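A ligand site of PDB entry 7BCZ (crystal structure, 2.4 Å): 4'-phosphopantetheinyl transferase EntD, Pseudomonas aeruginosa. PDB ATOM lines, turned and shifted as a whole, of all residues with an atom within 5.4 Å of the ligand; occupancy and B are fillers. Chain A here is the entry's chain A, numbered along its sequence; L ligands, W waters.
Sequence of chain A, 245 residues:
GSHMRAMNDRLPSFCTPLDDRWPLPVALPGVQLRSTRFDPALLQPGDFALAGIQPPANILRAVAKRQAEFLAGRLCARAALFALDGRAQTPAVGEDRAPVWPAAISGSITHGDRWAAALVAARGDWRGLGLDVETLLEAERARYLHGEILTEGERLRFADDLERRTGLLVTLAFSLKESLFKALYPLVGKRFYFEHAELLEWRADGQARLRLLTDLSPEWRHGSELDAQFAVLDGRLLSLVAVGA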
ATOM      1  N   ARG A  66     -29.727 -13.297 -31.211  1.00  0.00           N
ATOM      2  CA  ARG A  66     -29.238 -12.656 -30.000  1.00  0.00           C
ATOM      3  C   ARG A  66     -30.144 -11.498 -29.587  1.00  0.00           C
ATOM      4  O   ARG A  66     -30.411 -11.310 -28.390  1.00  0.00           O
ATOM      5  CB  ARG A  66     -27.804 -12.165 -30.222  1.00  0.00           C
ATOM      6  CG  ARG A  66     -27.249 -11.263 -29.129  1.00  0.00           C
ATOM      7  CD  ARG A  66     -27.364 -11.908 -27.755  1.00  0.00           C
ATOM      8  NE  ARG A  66     -26.839 -11.029 -26.708  1.00  0.00           N
ATOM      9  CZ  ARG A  66     -27.077 -11.189 -25.413  1.00  0.00           C
ATOM     10  NH1 ARG A  66     -27.828 -12.182 -24.982  1.00  0.00           N
ATOM     11  NH2 ARG A  66     -26.558 -10.339 -24.537  1.00  0.00           N
ATOM     12  N   GLU A  69     -33.281 -13.043 -27.880  1.00  0.00           N
ATOM     13  CA  GLU A  69     -32.962 -13.576 -26.553  1.00  0.00           C
ATOM     14  C   GLU A  69     -32.773 -12.457 -25.540  1.00  0.00           C
ATOM     15  O   GLU A  69     -33.348 -12.485 -24.449  1.00  0.00           O
ATOM     16  CB  GLU A  69     -31.704 -14.442 -26.625  1.00  0.00           C
ATOM     17  CG  GLU A  69     -31.885 -15.769 -27.337  1.00  0.00           C
ATOM     18  CD  GLU A  69     -30.594 -16.540 -27.435  1.00  0.00           C
ATOM     19  OE1 GLU A  69     -29.524 -15.907 -27.319  1.00  0.00           O
ATOM     20  OE2 GLU A  69     -30.634 -17.777 -27.625  1.00  0.00           O
ATOM     21  N   PHE A  70     -31.940 -11.461 -25.879  1.00  0.00           N
ATOM     22  CA  PHE A  70     -31.703 -10.354 -24.958  1.00  0.00           C
ATOM     23  C   PHE A  70     -33.009  -9.659 -24.580  1.00  0.00           C
ATOM     24  O   PHE A  70     -33.291  -9.476 -23.388  1.00  0.00           O
ATOM     25  CB  PHE A  70     -30.729  -9.353 -25.599  1.00  0.00           C
ATOM     26  CG  PHE A  70     -30.565  -8.087 -24.810  1.00  0.00           C
ATOM     27  CD1 PHE A  70     -29.524  -7.948 -23.903  1.00  0.00           C
ATOM     28  CD2 PHE A  70     -31.444  -7.019 -24.967  1.00  0.00           C
ATOM     29  CE1 PHE A  70     -29.367  -6.788 -23.175  1.00  0.00           C
ATOM     30  CE2 PHE A  70     -31.293  -5.854 -24.244  1.00  0.00           C
ATOM     31  CZ  PHE A  70     -30.251  -5.736 -23.342  1.00  0.00           C
ATOM     32  N   ARG A  74     -35.008  -9.484 -21.066  1.00  0.00           N
ATOM     33  CA  ARG A  74     -35.198  -8.197 -20.402  1.00  0.00           C
ATOM     34  C   ARG A  74     -36.662  -7.918 -20.096  1.00  0.00           C
ATOM     35  O   ARG A  74     -36.968  -7.236 -19.117  1.00  0.00           O
ATOM     36  CB  ARG A  74     -34.613  -7.070 -21.252  1.00  0.00           C
ATOM     37  CG  ARG A  74     -33.095  -7.018 -21.230  1.00  0.00           C
ATOM     38  CD  ARG A  74     -32.552  -7.241 -19.828  1.00  0.00           C
ATOM     39  NE  ARG A  74     -31.229  -6.672 -19.648  1.00  0.00           N
ATOM     40  CZ  ARG A  74     -30.096  -7.376 -19.580  1.00  0.00           C
ATOM     41  NH1 ARG A  74     -30.114  -8.693 -19.681  1.00  0.00           N
ATOM     42  NH2 ARG A  74     -28.950  -6.758 -19.418  1.00  0.00           N
ATOM     43  N   VAL A  93     -26.180  -3.757 -18.964  1.00  0.00           N
ATOM     44  CA  VAL A  93     -25.205  -4.799 -19.265  1.00  0.00           C
ATOM     45  C   VAL A  93     -23.857  -4.322 -18.742  1.00  0.00           C
ATOM     46  O   VAL A  93     -23.330  -3.292 -19.190  1.00  0.00           O
ATOM     47  CB  VAL A  93     -25.153  -5.103 -20.769  1.00  0.00           C
ATOM     48  CG1 VAL A  93     -24.027  -6.077 -21.068  1.00  0.00           C
ATOM     49  CG2 VAL A  93     -26.487  -5.663 -21.250  1.00  0.00           C
ATOM     50  N   ASP A  96     -18.398  -6.673 -17.360  1.00  0.00           N
ATOM     51  CA  ASP A  96     -18.145  -8.093 -17.199  1.00  0.00           C
ATOM     52  C   ASP A  96     -19.303  -8.945 -17.723  1.00  0.00           C
ATOM     53  O   ASP A  96     -19.408 -10.122 -17.337  1.00  0.00           O
ATOM     54  CB  ASP A  96     -17.880  -8.424 -15.728  1.00  0.00           C
ATOM     55  CG  ASP A  96     -19.052  -8.065 -14.837  1.00  0.00           C
ATOM     56  OD1 ASP A  96     -19.302  -8.801 -13.858  1.00  0.00           O
ATOM     57  OD2 ASP A  96     -19.736  -7.060 -15.126  1.00  0.00           O
ATOM     58  N   ARG A  97     -20.177  -8.373 -18.557  1.00  0.00           N
ATOM     59  CA  ARG A  97     -21.230  -9.086 -19.271  1.00  0.00           C
ATOM     60  C   ARG A  97     -22.385  -9.490 -18.360  1.00  0.00           C
ATOM     61  O   ARG A  97     -23.444  -9.927 -18.841  1.00  0.00           O
ATOM     62  CB  ARG A  97     -20.667 -10.321 -19.979  1.00  0.00           C
ATOM     63  CG  ARG A  97     -19.988 -10.025 -21.305  1.00  0.00           C
ATOM     64  CD  ARG A  97     -19.666 -11.310 -22.062  1.00  0.00           C
ATOM     65  NE  ARG A  97     -20.607 -11.567 -23.144  1.00  0.00           N
ATOM     66  CZ  ARG A  97     -21.720 -12.277 -23.021  1.00  0.00           C
ATOM     67  NH1 ARG A  97     -22.056 -12.796 -21.852  1.00  0.00           N
ATOM     68  NH2 ARG A  97     -22.506 -12.449 -24.073  1.00  0.00           N
ATOM     69  N   ALA A  98     -22.210  -9.374 -17.054  1.00  0.00           N
ATOM     70  CA  ALA A  98     -23.283  -9.668 -16.119  1.00  0.00           C
ATOM     71  C   ALA A  98     -24.317  -8.547 -16.108  1.00  0.00           C
ATOM     72  O   ALA A  98     -24.014  -7.397 -16.443  1.00  0.00           O
ATOM     73  CB  ALA A  98     -22.720  -9.871 -14.718  1.00  0.00           C
ATOM     74  N   PRO A  99     -25.553  -8.850 -15.732  1.00  0.00           N
ATOM     75  CA  PRO A  99     -26.544  -7.786 -15.547  1.00  0.00           C
ATOM     76  C   PRO A  99     -26.203  -6.914 -14.342  1.00  0.00           C
ATOM     77  O   PRO A  99     -25.600  -7.377 -13.377  1.00  0.00           O
ATOM     78  CB  PRO A  99     -27.861  -8.546 -15.322  1.00  0.00           C
ATOM     79  CG  PRO A  99     -27.430  -9.903 -14.835  1.00  0.00           C
ATOM     80  CD  PRO A  99     -26.148 -10.184 -15.556  1.00  0.00           C
ATOM     81  N   ILE A 109     -30.918 -14.100 -15.267  1.00  0.00           N
ATOM     82  CA  ILE A 109     -31.586 -14.190 -16.559  1.00  0.00           C
ATOM     83  C   ILE A 109     -31.042 -15.416 -17.291  1.00  0.00           C
ATOM     84  O   ILE A 109     -29.837 -15.700 -17.232  1.00  0.00           O
ATOM     85  CB  ILE A 109     -31.378 -12.912 -17.406  1.00  0.00           C
ATOM     86  CG1 ILE A 109     -32.017 -11.712 -16.708  1.00  0.00           C
ATOM     87  CG2 ILE A 109     -31.969 -13.073 -18.789  1.00  0.00           C
ATOM     88  CD1 ILE A 109     -31.571 -10.393 -17.275  1.00  0.00           C
ATOM     89  N   THR A 110     -31.940 -16.153 -17.942  1.00  0.00           N
ATOM     90  CA  THR A 110     -31.551 -17.249 -18.821  1.00  0.00           C
ATOM     91  C   THR A 110     -32.458 -17.224 -20.040  1.00  0.00           C
ATOM     92  O   THR A 110     -33.584 -16.734 -19.997  1.00  0.00           O
ATOM     93  CB  THR A 110     -31.626 -18.605 -18.094  1.00  0.00           C
ATOM     94  OG1 THR A 110     -31.024 -19.622 -18.902  1.00  0.00           O
ATOM     95  CG2 THR A 110     -33.053 -18.989 -17.777  1.00  0.00           C
ATOM     96  N   HIS A 111     -31.926 -17.727 -21.154  1.00  0.00           N
ATOM     97  CA  HIS A 111     -32.697 -17.820 -22.382  1.00  0.00           C
ATOM     98  C   HIS A 111     -32.021 -18.807 -23.318  1.00  0.00           C
ATOM     99  O   HIS A 111     -30.813 -18.711 -23.543  1.00  0.00           O
ATOM    100  CB  HIS A 111     -32.861 -16.451 -23.050  1.00  0.00           C
ATOM    101  CG  HIS A 111     -31.661 -15.558 -22.932  1.00  0.00           C
ATOM    102  ND1 HIS A 111     -30.380 -15.993 -23.209  1.00  0.00           N
ATOM    103  CD2 HIS A 111     -31.552 -14.253 -22.577  1.00  0.00           C
ATOM    104  CE1 HIS A 111     -29.530 -14.984 -23.029  1.00  0.00           C
ATOM    105  NE2 HIS A 111     -30.221 -13.924 -22.649  1.00  0.00           N
ATOM    106  N   GLY A 112     -32.806 -19.744 -23.848  1.00  0.00           N
ATOM    107  CA  GLY A 112     -32.250 -20.767 -24.701  1.00  0.00           C
ATOM    108  C   GLY A 112     -32.931 -20.855 -26.046  1.00  0.00           C
ATOM    109  O   GLY A 112     -33.128 -19.845 -26.719  1.00  0.00           O
ATOM    110  N   LEU A 131     -30.049 -18.848 -12.366  1.00  0.00           N
ATOM    111  CA  LEU A 131     -31.041 -19.605 -13.114  1.00  0.00           C
ATOM    112  C   LEU A 131     -30.446 -19.961 -14.469  1.00  0.00           C
ATOM    113  O   LEU A 131     -29.776 -19.133 -15.096  1.00  0.00           O
ATOM    114  CB  LEU A 131     -32.326 -18.790 -13.282  1.00  0.00           C
ATOM    115  CG  LEU A 131     -33.603 -19.461 -13.806  1.00  0.00           C
ATOM    116  CD1 LEU A 131     -34.164 -20.422 -12.771  1.00  0.00           C
ATOM    117  CD2 LEU A 131     -34.625 -18.408 -14.192  1.00  0.00           C
ATOM    118  N   ASP A 132     -30.693 -21.180 -14.930  1.00  0.00           N
ATOM    119  CA  ASP A 132     -30.176 -21.576 -16.231  1.00  0.00           C
ATOM    120  C   ASP A 132     -31.011 -22.696 -16.818  1.00  0.00           C
ATOM    121  O   ASP A 132     -31.298 -23.678 -16.137  1.00  0.00           O
ATOM    122  CB  ASP A 132     -28.705 -22.016 -16.140  1.00  0.00           C
ATOM    123  CG  ASP A 132     -28.129 -22.384 -17.489  1.00  0.00           C
ATOM    124  OD1 ASP A 132     -28.449 -23.470 -18.005  1.00  0.00           O
ATOM    125  OD2 ASP A 132     -27.386 -21.557 -18.053  1.00  0.00           O
ATOM    126  N   VAL A 133     -31.368 -22.537 -18.092  1.00  0.00           N
ATOM    127  CA  VAL A 133     -32.068 -23.569 -18.844  1.00  0.00           C
ATOM    128  C   VAL A 133     -31.152 -24.060 -19.949  1.00  0.00           C
ATOM    129  O   VAL A 133     -30.321 -23.311 -20.471  1.00  0.00           O
ATOM    130  CB  VAL A 133     -33.422 -23.054 -19.401  1.00  0.00           C
ATOM    131  CG1 VAL A 133     -33.213 -21.989 -20.483  1.00  0.00           C
ATOM    132  CG2 VAL A 133     -34.256 -24.224 -19.917  1.00  0.00           C
ATOM    133  N   GLU A 134     -31.273 -25.352 -20.281  1.00  0.00           N
ATOM    134  CA  GLU A 134     -30.481 -25.975 -21.323  1.00  0.00           C
ATOM    135  C   GLU A 134     -31.299 -27.057 -21.992  1.00  0.00           C
ATOM    136  O   GLU A 134     -31.985 -27.836 -21.320  1.00  0.00           O
ATOM    137  CB  GLU A 134     -29.189 -26.579 -20.757  1.00  0.00           C
ATOM    138  CG  GLU A 134     -28.153 -25.557 -20.341  1.00  0.00           C
ATOM    139  CD  GLU A 134     -27.682 -24.681 -21.489  1.00  0.00           C
ATOM    140  OE1 GLU A 134     -27.444 -23.472 -21.265  1.00  0.00           O
ATOM    141  OE2 GLU A 134     -27.559 -25.203 -22.610  1.00  0.00           O
ATOM    142  N   LYS A 177     -24.212 -26.386 -12.848  1.00  0.00           N
ATOM    143  CA  LYS A 177     -22.933 -25.683 -12.701  1.00  0.00           C
ATOM    144  C   LYS A 177     -22.996 -24.270 -13.273  1.00  0.00           C
ATOM    145  O   LYS A 177     -22.316 -23.368 -12.759  1.00  0.00           O
ATOM    146  CB  LYS A 177     -21.814 -26.472 -13.358  1.00  0.00           C
ATOM    147  CG  LYS A 177     -21.473 -27.757 -12.630  1.00  0.00           C
ATOM    148  CD  LYS A 177     -20.213 -28.381 -13.167  1.00  0.00           C
ATOM    149  CE  LYS A 177     -19.925 -29.695 -12.466  1.00  0.00           C
ATOM    150  NZ  LYS A 177     -18.682 -30.272 -12.993  1.00  0.00           N
ATOM    151  N   GLU A 178     -23.786 -24.055 -14.326  1.00  0.00           N
ATOM    152  CA  GLU A 178     -23.945 -22.695 -14.838  1.00  0.00           C
ATOM    153  C   GLU A 178     -24.768 -21.841 -13.885  1.00  0.00           C
ATOM    154  O   GLU A 178     -24.472 -20.662 -13.695  1.00  0.00           O
ATOM    155  CB  GLU A 178     -24.560 -22.731 -16.231  1.00  0.00           C
ATOM    156  CG  GLU A 178     -23.628 -23.296 -17.287  1.00  0.00           C
ATOM    157  CD  GLU A 178     -24.046 -22.938 -18.700  1.00  0.00           C
ATOM    158  OE1 GLU A 178     -25.238 -23.112 -19.021  1.00  0.00           O
ATOM    159  OE2 GLU A 178     -23.187 -22.490 -19.483  1.00  0.00           O
ATOM    160  N   LEU A 180     -24.964 -22.336 -10.568  1.00  0.00           N
ATOM    161  CA  LEU A 180     -24.052 -22.107  -9.450  1.00  0.00           C
ATOM    162  C   LEU A 180     -23.092 -20.967  -9.743  1.00  0.00           C
ATOM    163  O   LEU A 180     -22.844 -20.116  -8.889  1.00  0.00           O
ATOM    164  CB  LEU A 180     -23.276 -23.388  -9.158  1.00  0.00           C
ATOM    165  CG  LEU A 180     -22.162 -23.328  -8.128  1.00  0.00           C
ATOM    166  CD1 LEU A 180     -22.731 -23.249  -6.723  1.00  0.00           C
ATOM    167  CD2 LEU A 180     -21.277 -24.536  -8.296  1.00  0.00           C
ATOM    168  N   PHE A 181     -22.556 -20.925 -10.966  1.00  0.00           N
ATOM    169  CA  PHE A 181     -21.719 -19.806 -11.379  1.00  0.00           C
ATOM    170  C   PHE A 181     -22.476 -18.480 -11.291  1.00  0.00           C
ATOM    171  O   PHE A 181     -21.999 -17.517 -10.673  1.00  0.00           O
ATOM    172  CB  PHE A 181     -21.200 -20.037 -12.796  1.00  0.00           C
ATOM    173  CG  PHE A 181     -20.378 -18.897 -13.342  1.00  0.00           C
ATOM    174  CD1 PHE A 181     -19.035 -18.786 -13.008  1.00  0.00           C
ATOM    175  CD2 PHE A 181     -20.936 -17.950 -14.178  1.00  0.00           C
ATOM    176  CE1 PHE A 181     -18.270 -17.746 -13.493  1.00  0.00           C
ATOM    177  CE2 PHE A 181     -20.181 -16.892 -14.669  1.00  0.00           C
ATOM    178  CZ  PHE A 181     -18.843 -16.796 -14.329  1.00  0.00           C
ATOM    179  N   LYS A 182     -23.664 -18.406 -11.903  1.00  0.00           N
ATOM    180  CA  LYS A 182     -24.430 -17.166 -11.922  1.00  0.00           C
ATOM    181  C   LYS A 182     -24.883 -16.722 -10.536  1.00  0.00           C
ATOM    182  O   LYS A 182     -25.132 -15.523 -10.337  1.00  0.00           O
ATOM    183  CB  LYS A 182     -25.657 -17.318 -12.845  1.00  0.00           C
ATOM    184  CG  LYS A 182     -25.318 -17.589 -14.294  1.00  0.00           C
ATOM    185  CD  LYS A 182     -26.508 -18.185 -15.034  1.00  0.00           C
ATOM    186  CE  LYS A 182     -27.274 -17.115 -15.804  1.00  0.00           C
ATOM    187  NZ  LYS A 182     -28.280 -17.713 -16.725  1.00  0.00           N
ATOM    188  N   TYR A 185     -21.060 -15.638  -8.657  1.00  0.00           N
ATOM    189  CA  TYR A 185     -20.176 -14.645  -9.267  1.00  0.00           C
ATOM    190  C   TYR A 185     -20.412 -13.234  -8.729  1.00  0.00           C
ATOM    191  O   TYR A 185     -19.417 -12.577  -8.365  1.00  0.00           O
ATOM    192  CB  TYR A 185     -20.308 -14.683 -10.796  1.00  0.00           C
ATOM    193  CG  TYR A 185     -19.360 -13.727 -11.487  1.00  0.00           C
ATOM    194  CD1 TYR A 185     -19.765 -12.432 -11.805  1.00  0.00           C
ATOM    195  CD2 TYR A 185     -18.072 -14.111 -11.806  1.00  0.00           C
ATOM    196  CE1 TYR A 185     -18.904 -11.547 -12.429  1.00  0.00           C
ATOM    197  CE2 TYR A 185     -17.196 -13.230 -12.431  1.00  0.00           C
ATOM    198  CZ  TYR A 185     -17.616 -11.960 -12.742  1.00  0.00           C
ATOM    199  OH  TYR A 185     -16.748 -11.081 -13.360  1.00  0.00           O
ATOM    200  N   PRO A 186     -21.635 -12.696  -8.664  1.00  0.00           N
ATOM    201  CA  PRO A 186     -21.802 -11.354  -8.089  1.00  0.00           C
ATOM    202  C   PRO A 186     -21.452 -11.267  -6.610  1.00  0.00           C
ATOM    203  O   PRO A 186     -21.541 -10.176  -6.027  1.00  0.00           O
ATOM    204  CB  PRO A 186     -23.294 -11.048  -8.320  1.00  0.00           C
ATOM    205  CG  PRO A 186     -23.706 -11.965  -9.431  1.00  0.00           C
ATOM    206  CD  PRO A 186     -22.906 -13.211  -9.198  1.00  0.00           C
ATOM    207  N   ARG A 191     -13.701 -15.918 -11.331  1.00  0.00           N
ATOM    208  CA  ARG A 191     -14.280 -16.752 -12.368  1.00  0.00           C
ATOM    209  C   ARG A 191     -13.864 -18.194 -12.133  1.00  0.00           C
ATOM    210  O   ARG A 191     -12.673 -18.501 -11.997  1.00  0.00           O
ATOM    211  CB  ARG A 191     -13.845 -16.303 -13.767  1.00  0.00           C
ATOM    212  CG  ARG A 191     -14.812 -15.348 -14.433  1.00  0.00           C
ATOM    213  CD  ARG A 191     -14.345 -14.970 -15.829  1.00  0.00           C
ATOM    214  NE  ARG A 191     -15.151 -13.882 -16.392  1.00  0.00           N
ATOM    215  CZ  ARG A 191     -16.283 -14.030 -17.067  1.00  0.00           C
ATOM    216  NH1 ARG A 191     -16.811 -15.227 -17.301  1.00  0.00           N
ATOM    217  NH2 ARG A 191     -16.909 -12.950 -17.526  1.00  0.00           N
ATOM    218  N   PHE A 192     -14.856 -19.079 -12.073  1.00  0.00           N
ATOM    219  CA  PHE A 192     -14.621 -20.512 -11.941  1.00  0.00           C
ATOM    220  C   PHE A 192     -15.396 -21.231 -13.032  1.00  0.00           C
ATOM    221  O   PHE A 192     -16.364 -20.704 -13.598  1.00  0.00           O
ATOM    222  CB  PHE A 192     -14.996 -21.033 -10.534  1.00  0.00           C
ATOM    223  CG  PHE A 192     -16.390 -20.688 -10.080  1.00  0.00           C
ATOM    224  CD1 PHE A 192     -16.742 -19.381  -9.780  1.00  0.00           C
ATOM    225  CD2 PHE A 192     -17.346 -21.676  -9.902  1.00  0.00           C
ATOM    226  CE1 PHE A 192     -18.010 -19.054  -9.349  1.00  0.00           C
ATOM    227  CE2 PHE A 192     -18.620 -21.373  -9.470  1.00  0.00           C
ATOM    228  CZ  PHE A 192     -18.948 -20.061  -9.188  1.00  0.00           C
ATOM    229  N   TYR A 193     -14.951 -22.441 -13.347  1.00  0.00           N
ATOM    230  CA  TYR A 193     -15.466 -23.145 -14.511  1.00  0.00           C
ATOM    231  C   TYR A 193     -15.915 -24.559 -14.149  1.00  0.00           C
ATOM    232  O   TYR A 193     -16.064 -24.875 -12.970  1.00  0.00           O
ATOM    233  CB  TYR A 193     -14.405 -23.167 -15.615  1.00  0.00           C
ATOM    234  CG  TYR A 193     -13.919 -21.779 -15.953  1.00  0.00           C
ATOM    235  CD1 TYR A 193     -14.611 -20.971 -16.859  1.00  0.00           C
ATOM    236  CD2 TYR A 193     -12.789 -21.239 -15.343  1.00  0.00           C
ATOM    237  CE1 TYR A 193     -14.177 -19.691 -17.164  1.00  0.00           C
ATOM    238  CE2 TYR A 193     -12.349 -19.964 -15.642  1.00  0.00           C
ATOM    239  CZ  TYR A 193     -13.044 -19.194 -16.547  1.00  0.00           C
ATOM    240  OH  TYR A 193     -12.613 -17.929 -16.846  1.00  0.00           O
ATOM    241  N   PHE A 194     -16.141 -25.388 -15.171  1.00  0.00           N
ATOM    242  CA  PHE A 194     -16.793 -26.684 -14.956  1.00  0.00           C
ATOM    243  C   PHE A 194     -15.991 -27.572 -14.014  1.00  0.00           C
ATOM    244  O   PHE A 194     -16.576 -28.358 -13.261  1.00  0.00           O
ATOM    245  CB  PHE A 194     -17.028 -27.366 -16.301  1.00  0.00           C
ATOM    246  CG  PHE A 194     -18.107 -26.737 -17.135  1.00  0.00           C
ATOM    247  CD1 PHE A 194     -19.334 -26.418 -16.583  1.00  0.00           C
ATOM    248  CD2 PHE A 194     -17.884 -26.443 -18.475  1.00  0.00           C
ATOM    249  CE1 PHE A 194     -20.335 -25.825 -17.341  1.00  0.00           C
ATOM    250  CE2 PHE A 194     -18.877 -25.849 -19.239  1.00  0.00           C
ATOM    251  CZ  PHE A 194     -20.107 -25.545 -18.680  1.00  0.00           C
ATOM    252  N   HIS A 196     -14.254 -26.650 -11.404  1.00  0.00           N
ATOM    253  CA  HIS A 196     -14.177 -26.119 -10.048  1.00  0.00           C
ATOM    254  C   HIS A 196     -15.377 -26.448  -9.174  1.00  0.00           C
ATOM    255  O   HIS A 196     -15.432 -25.973  -8.028  1.00  0.00           O
ATOM    256  CB  HIS A 196     -13.972 -24.606 -10.111  1.00  0.00           C
ATOM    257  CG  HIS A 196     -12.676 -24.193 -10.745  1.00  0.00           C
ATOM    258  ND1 HIS A 196     -12.588 -23.138 -11.619  1.00  0.00           N
ATOM    259  CD2 HIS A 196     -11.431 -24.707 -10.639  1.00  0.00           C
ATOM    260  CE1 HIS A 196     -11.335 -23.015 -12.030  1.00  0.00           C
ATOM    261  NE2 HIS A 196     -10.611 -23.948 -11.443  1.00  0.00           N
ATOM    262  N   ALA A 197     -16.341 -27.233  -9.655  1.00  0.00           N
ATOM    263  CA  ALA A 197     -17.448 -27.678  -8.830  1.00  0.00           C
ATOM    264  C   ALA A 197     -17.835 -29.086  -9.231  1.00  0.00           C
ATOM    265  O   ALA A 197     -17.522 -29.529 -10.345  1.00  0.00           O
ATOM    266  CB  ALA A 197     -18.650 -26.745  -8.934  1.00  0.00           C
HETATM  267  N1  LIG L   1     -22.680 -13.628 -13.628  1.00  0.00           N
HETATM  268  C1  LIG L   1     -24.062 -13.719 -13.668  1.00  0.00           C
HETATM  269  N2  LIG L   1     -24.919 -13.697 -14.703  1.00  0.00           N
HETATM  270  C2  LIG L   1     -24.261 -13.556 -15.919  1.00  0.00           C
HETATM  271  C3  LIG L   1     -22.842 -13.439 -16.043  1.00  0.00           C
HETATM  272  C4  LIG L   1     -22.073 -13.486 -14.845  1.00  0.00           C
HETATM  273  N3  LIG L   1     -20.707 -13.374 -14.904  1.00  0.00           N
HETATM  274  N4  LIG L   1     -22.466 -13.310 -17.384  1.00  0.00           N
HETATM  275  C5  LIG L   1     -23.632 -13.343 -18.051  1.00  0.00           C
HETATM  276  N5  LIG L   1     -24.743 -13.482 -17.218  1.00  0.00           N
HETATM  277  C6  LIG L   1     -26.172 -13.560 -17.657  1.00  0.00           C
HETATM  278  C7  LIG L   1     -26.492 -12.441 -18.697  1.00  0.00           C
HETATM  279  O1  LIG L   1     -27.529 -11.623 -18.278  1.00  0.00           O
HETATM  280  C8  LIG L   1     -26.964 -13.311 -19.924  1.00  0.00           C
HETATM  281  O2  LIG L   1     -28.115 -12.808 -20.418  1.00  0.00           O
HETATM  282  P1  LIG L   1     -27.821 -11.355 -21.503  1.00  0.00           P
HETATM  283  O3  LIG L   1     -28.147 -10.347 -20.465  1.00  0.00           O
HETATM  284  O4  LIG L   1     -26.356 -11.498 -21.918  1.00  0.00           O
HETATM  285  O5  LIG L   1     -28.880 -11.612 -22.556  1.00  0.00           O
HETATM  286  C9  LIG L   1     -27.264 -14.663 -19.259  1.00  0.00           C
HETATM  287  O6  LIG L   1     -26.305 -14.820 -18.249  1.00  0.00           O
HETATM  288  C10 LIG L   1     -27.156 -15.820 -20.227  1.00  0.00           C
HETATM  289  O7  LIG L   1     -27.504 -16.969 -19.493  1.00  0.00           O
HETATM  290  P2  LIG L   1     -27.737 -18.118 -20.609  1.00  0.00           P
HETATM  291  O8  LIG L   1     -28.519 -17.530 -21.703  1.00  0.00           O
HETATM  292  O9  LIG L   1     -28.208 -19.420 -20.002  1.00  0.00           O
HETATM  293  O10 LIG L   1     -26.219 -18.259 -21.377  1.00  0.00           O
HETATM  294  P3  LIG L   1     -25.476 -19.657 -21.081  1.00  0.00           P
HETATM  295  O11 LIG L   1     -25.990 -20.368 -19.904  1.00  0.00           O
HETATM  296  O12 LIG L   1     -25.122 -20.408 -22.341  1.00  0.00           O
HETATM  297  O13 LIG L   1     -23.938 -19.157 -20.484  1.00  0.00           O
HETATM  298  C11 LIG L   1     -22.915 -18.196 -18.611  1.00  0.00           C
HETATM  299  C12 LIG L   1     -24.202 -18.322 -19.418  1.00  0.00           C
HETATM  300  C13 LIG L   1     -22.867 -16.846 -17.934  1.00  0.00           C
HETATM  301  C14 LIG L   1     -22.853 -19.317 -17.592  1.00  0.00           C
HETATM  302  C15 LIG L   1     -21.751 -18.319 -19.625  1.00  0.00           C
HETATM  303  O14 LIG L   1     -21.532 -17.106 -20.291  1.00  0.00           O
HETATM  304  C16 LIG L   1     -20.416 -18.711 -18.951  1.00  0.00           C
HETATM  305  O15 LIG L   1     -19.653 -17.855 -18.511  1.00  0.00           O
HETATM  306  N6  LIG L   1     -20.102 -20.075 -18.897  1.00  0.00           N
HETATM  307  C17 LIG L   1     -18.861 -20.514 -18.278  1.00  0.00           C
HETATM  308  C18 LIG L   1     -18.984 -20.389 -16.756  1.00  0.00           C
HETATM  309  C19 LIG L   1     -19.379 -21.739 -16.200  1.00  0.00           C
HETATM  310  O16 LIG L   1     -20.101 -22.551 -16.758  1.00  0.00           O
HETATM  311  N7  LIG L   1     -18.866 -22.019 -14.941  1.00  0.00           N
HETATM  312  C20 LIG L   1     -19.174 -23.292 -14.279  1.00  0.00           C
HETATM  313  C21 LIG L   1     -19.001 -23.075 -12.773  1.00  0.00           C
HETATM  314  S1  LIG L   1     -19.178 -24.643 -11.877  1.00  0.00           S
HETATM  315  O   HOH W   1     -31.623 -10.619 -21.473  1.00  0.00           O
HETATM  316  O   HOH W   2     -26.529  -8.320 -18.937  1.00  0.00           O
HETATM  317  O   HOH W   3     -27.515 -14.381 -14.039  1.00  0.00           O
HETATM  318  O   HOH W   4     -24.548 -16.646 -22.065  1.00  0.00           O
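An oxygen (O7) of the ligand lies close to the backbone carbonyl oxygen of Ile 109 (3.5 Å).
Merely in contact with the ligand: Phe 70 (3.9 Å), Arg 97 (3.5 Å), Ala 98 (3.7 Å), Pro 99 (3.4 Å), Glu 134 (3.7 Å), Phe 181 (3.6 Å), Tyr 185 (3.4 Å), Phe 194 (3.3 Å) and Ala 197 (3.7 Å).
NZ of Lys 182 lies within salt-bridge range of O9 of the ligand (3.7 Å).
The guanidinium group (NH1) of Arg 74 lies within salt-bridge range of an oxygen (O3) of the ligand.
An oxygen (O11) of the ligand lies close to the side-chain carboxylate (OD2) of Asp 132 (2.6 Å).
The side-chain carboxylate (OE1) of Glu 178 sits close to an oxygen (O11) of the ligand, 3.0 Å away.
OG1 of Thr 110 lies within hydrogen-bond range of O9 of the ligand (3.0 Å).
An oxygen (O5) of the ligand is in salt-bridge range of the guanidinium group of Arg 66, at 2.7 Å.
The backbone carbonyl oxygen (O) of Lys 177 sits close to a sulfur (S1) of the ligand (3.5 Å).
O of Tyr 193 lies close to S1 of the ligand, at 3.3 Å.
The backbone NH (N) of His 111 lies close to an oxygen (O8) of the ligand, at 3.5 Å.
NE2 of His 111 is in hydrogen-bond range of O5 of the ligand (2.7 Å).
The backbone carbonyl oxygen (O) of Phe 192 is in hydrogen-bond range of a nitrogen (N7) of the ligand (3.1 Å).
Water W2 lies within hydrogen-bond range of NH2 of Arg 74, O3 of the ligand and O of Arg 97.
Water W1 lies within hydrogen-bond range of O of Phe 70 (2.8 Å), NH1 of Arg 74 (3.0 Å) and O5 of the ligand (3.1 Å).
The side-chain amino group of Lys 182 lies within hydrogen-bond range of the backbone carbonyl oxygen of Ile 109.
NZ of Lys 177 sits at hydrogen-bond distance from O of Ala 197 (3.0 Å).
The side-chain amino group (NZ) of Lys 177 is in hydrogen-bond range of the backbone carbonyl oxygen (O) of Phe 194 (2.9 Å).
The side-chain carboxylate (OD1) of Asp 96 sits close to the side-chain hydroxyl (OH) of Tyr 185 (3.5 Å).
N of Tyr 193 is in hydrogen-bond range of ND1 of His 196 (3.0 Å).
The side-chain hydroxyl of Thr 110 lies within hydrogen-bond range of the backbone NH of Val 133.
O of Leu 131 sits at hydrogen-bond distance from NZ of Lys 182, 2.6 Å away.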
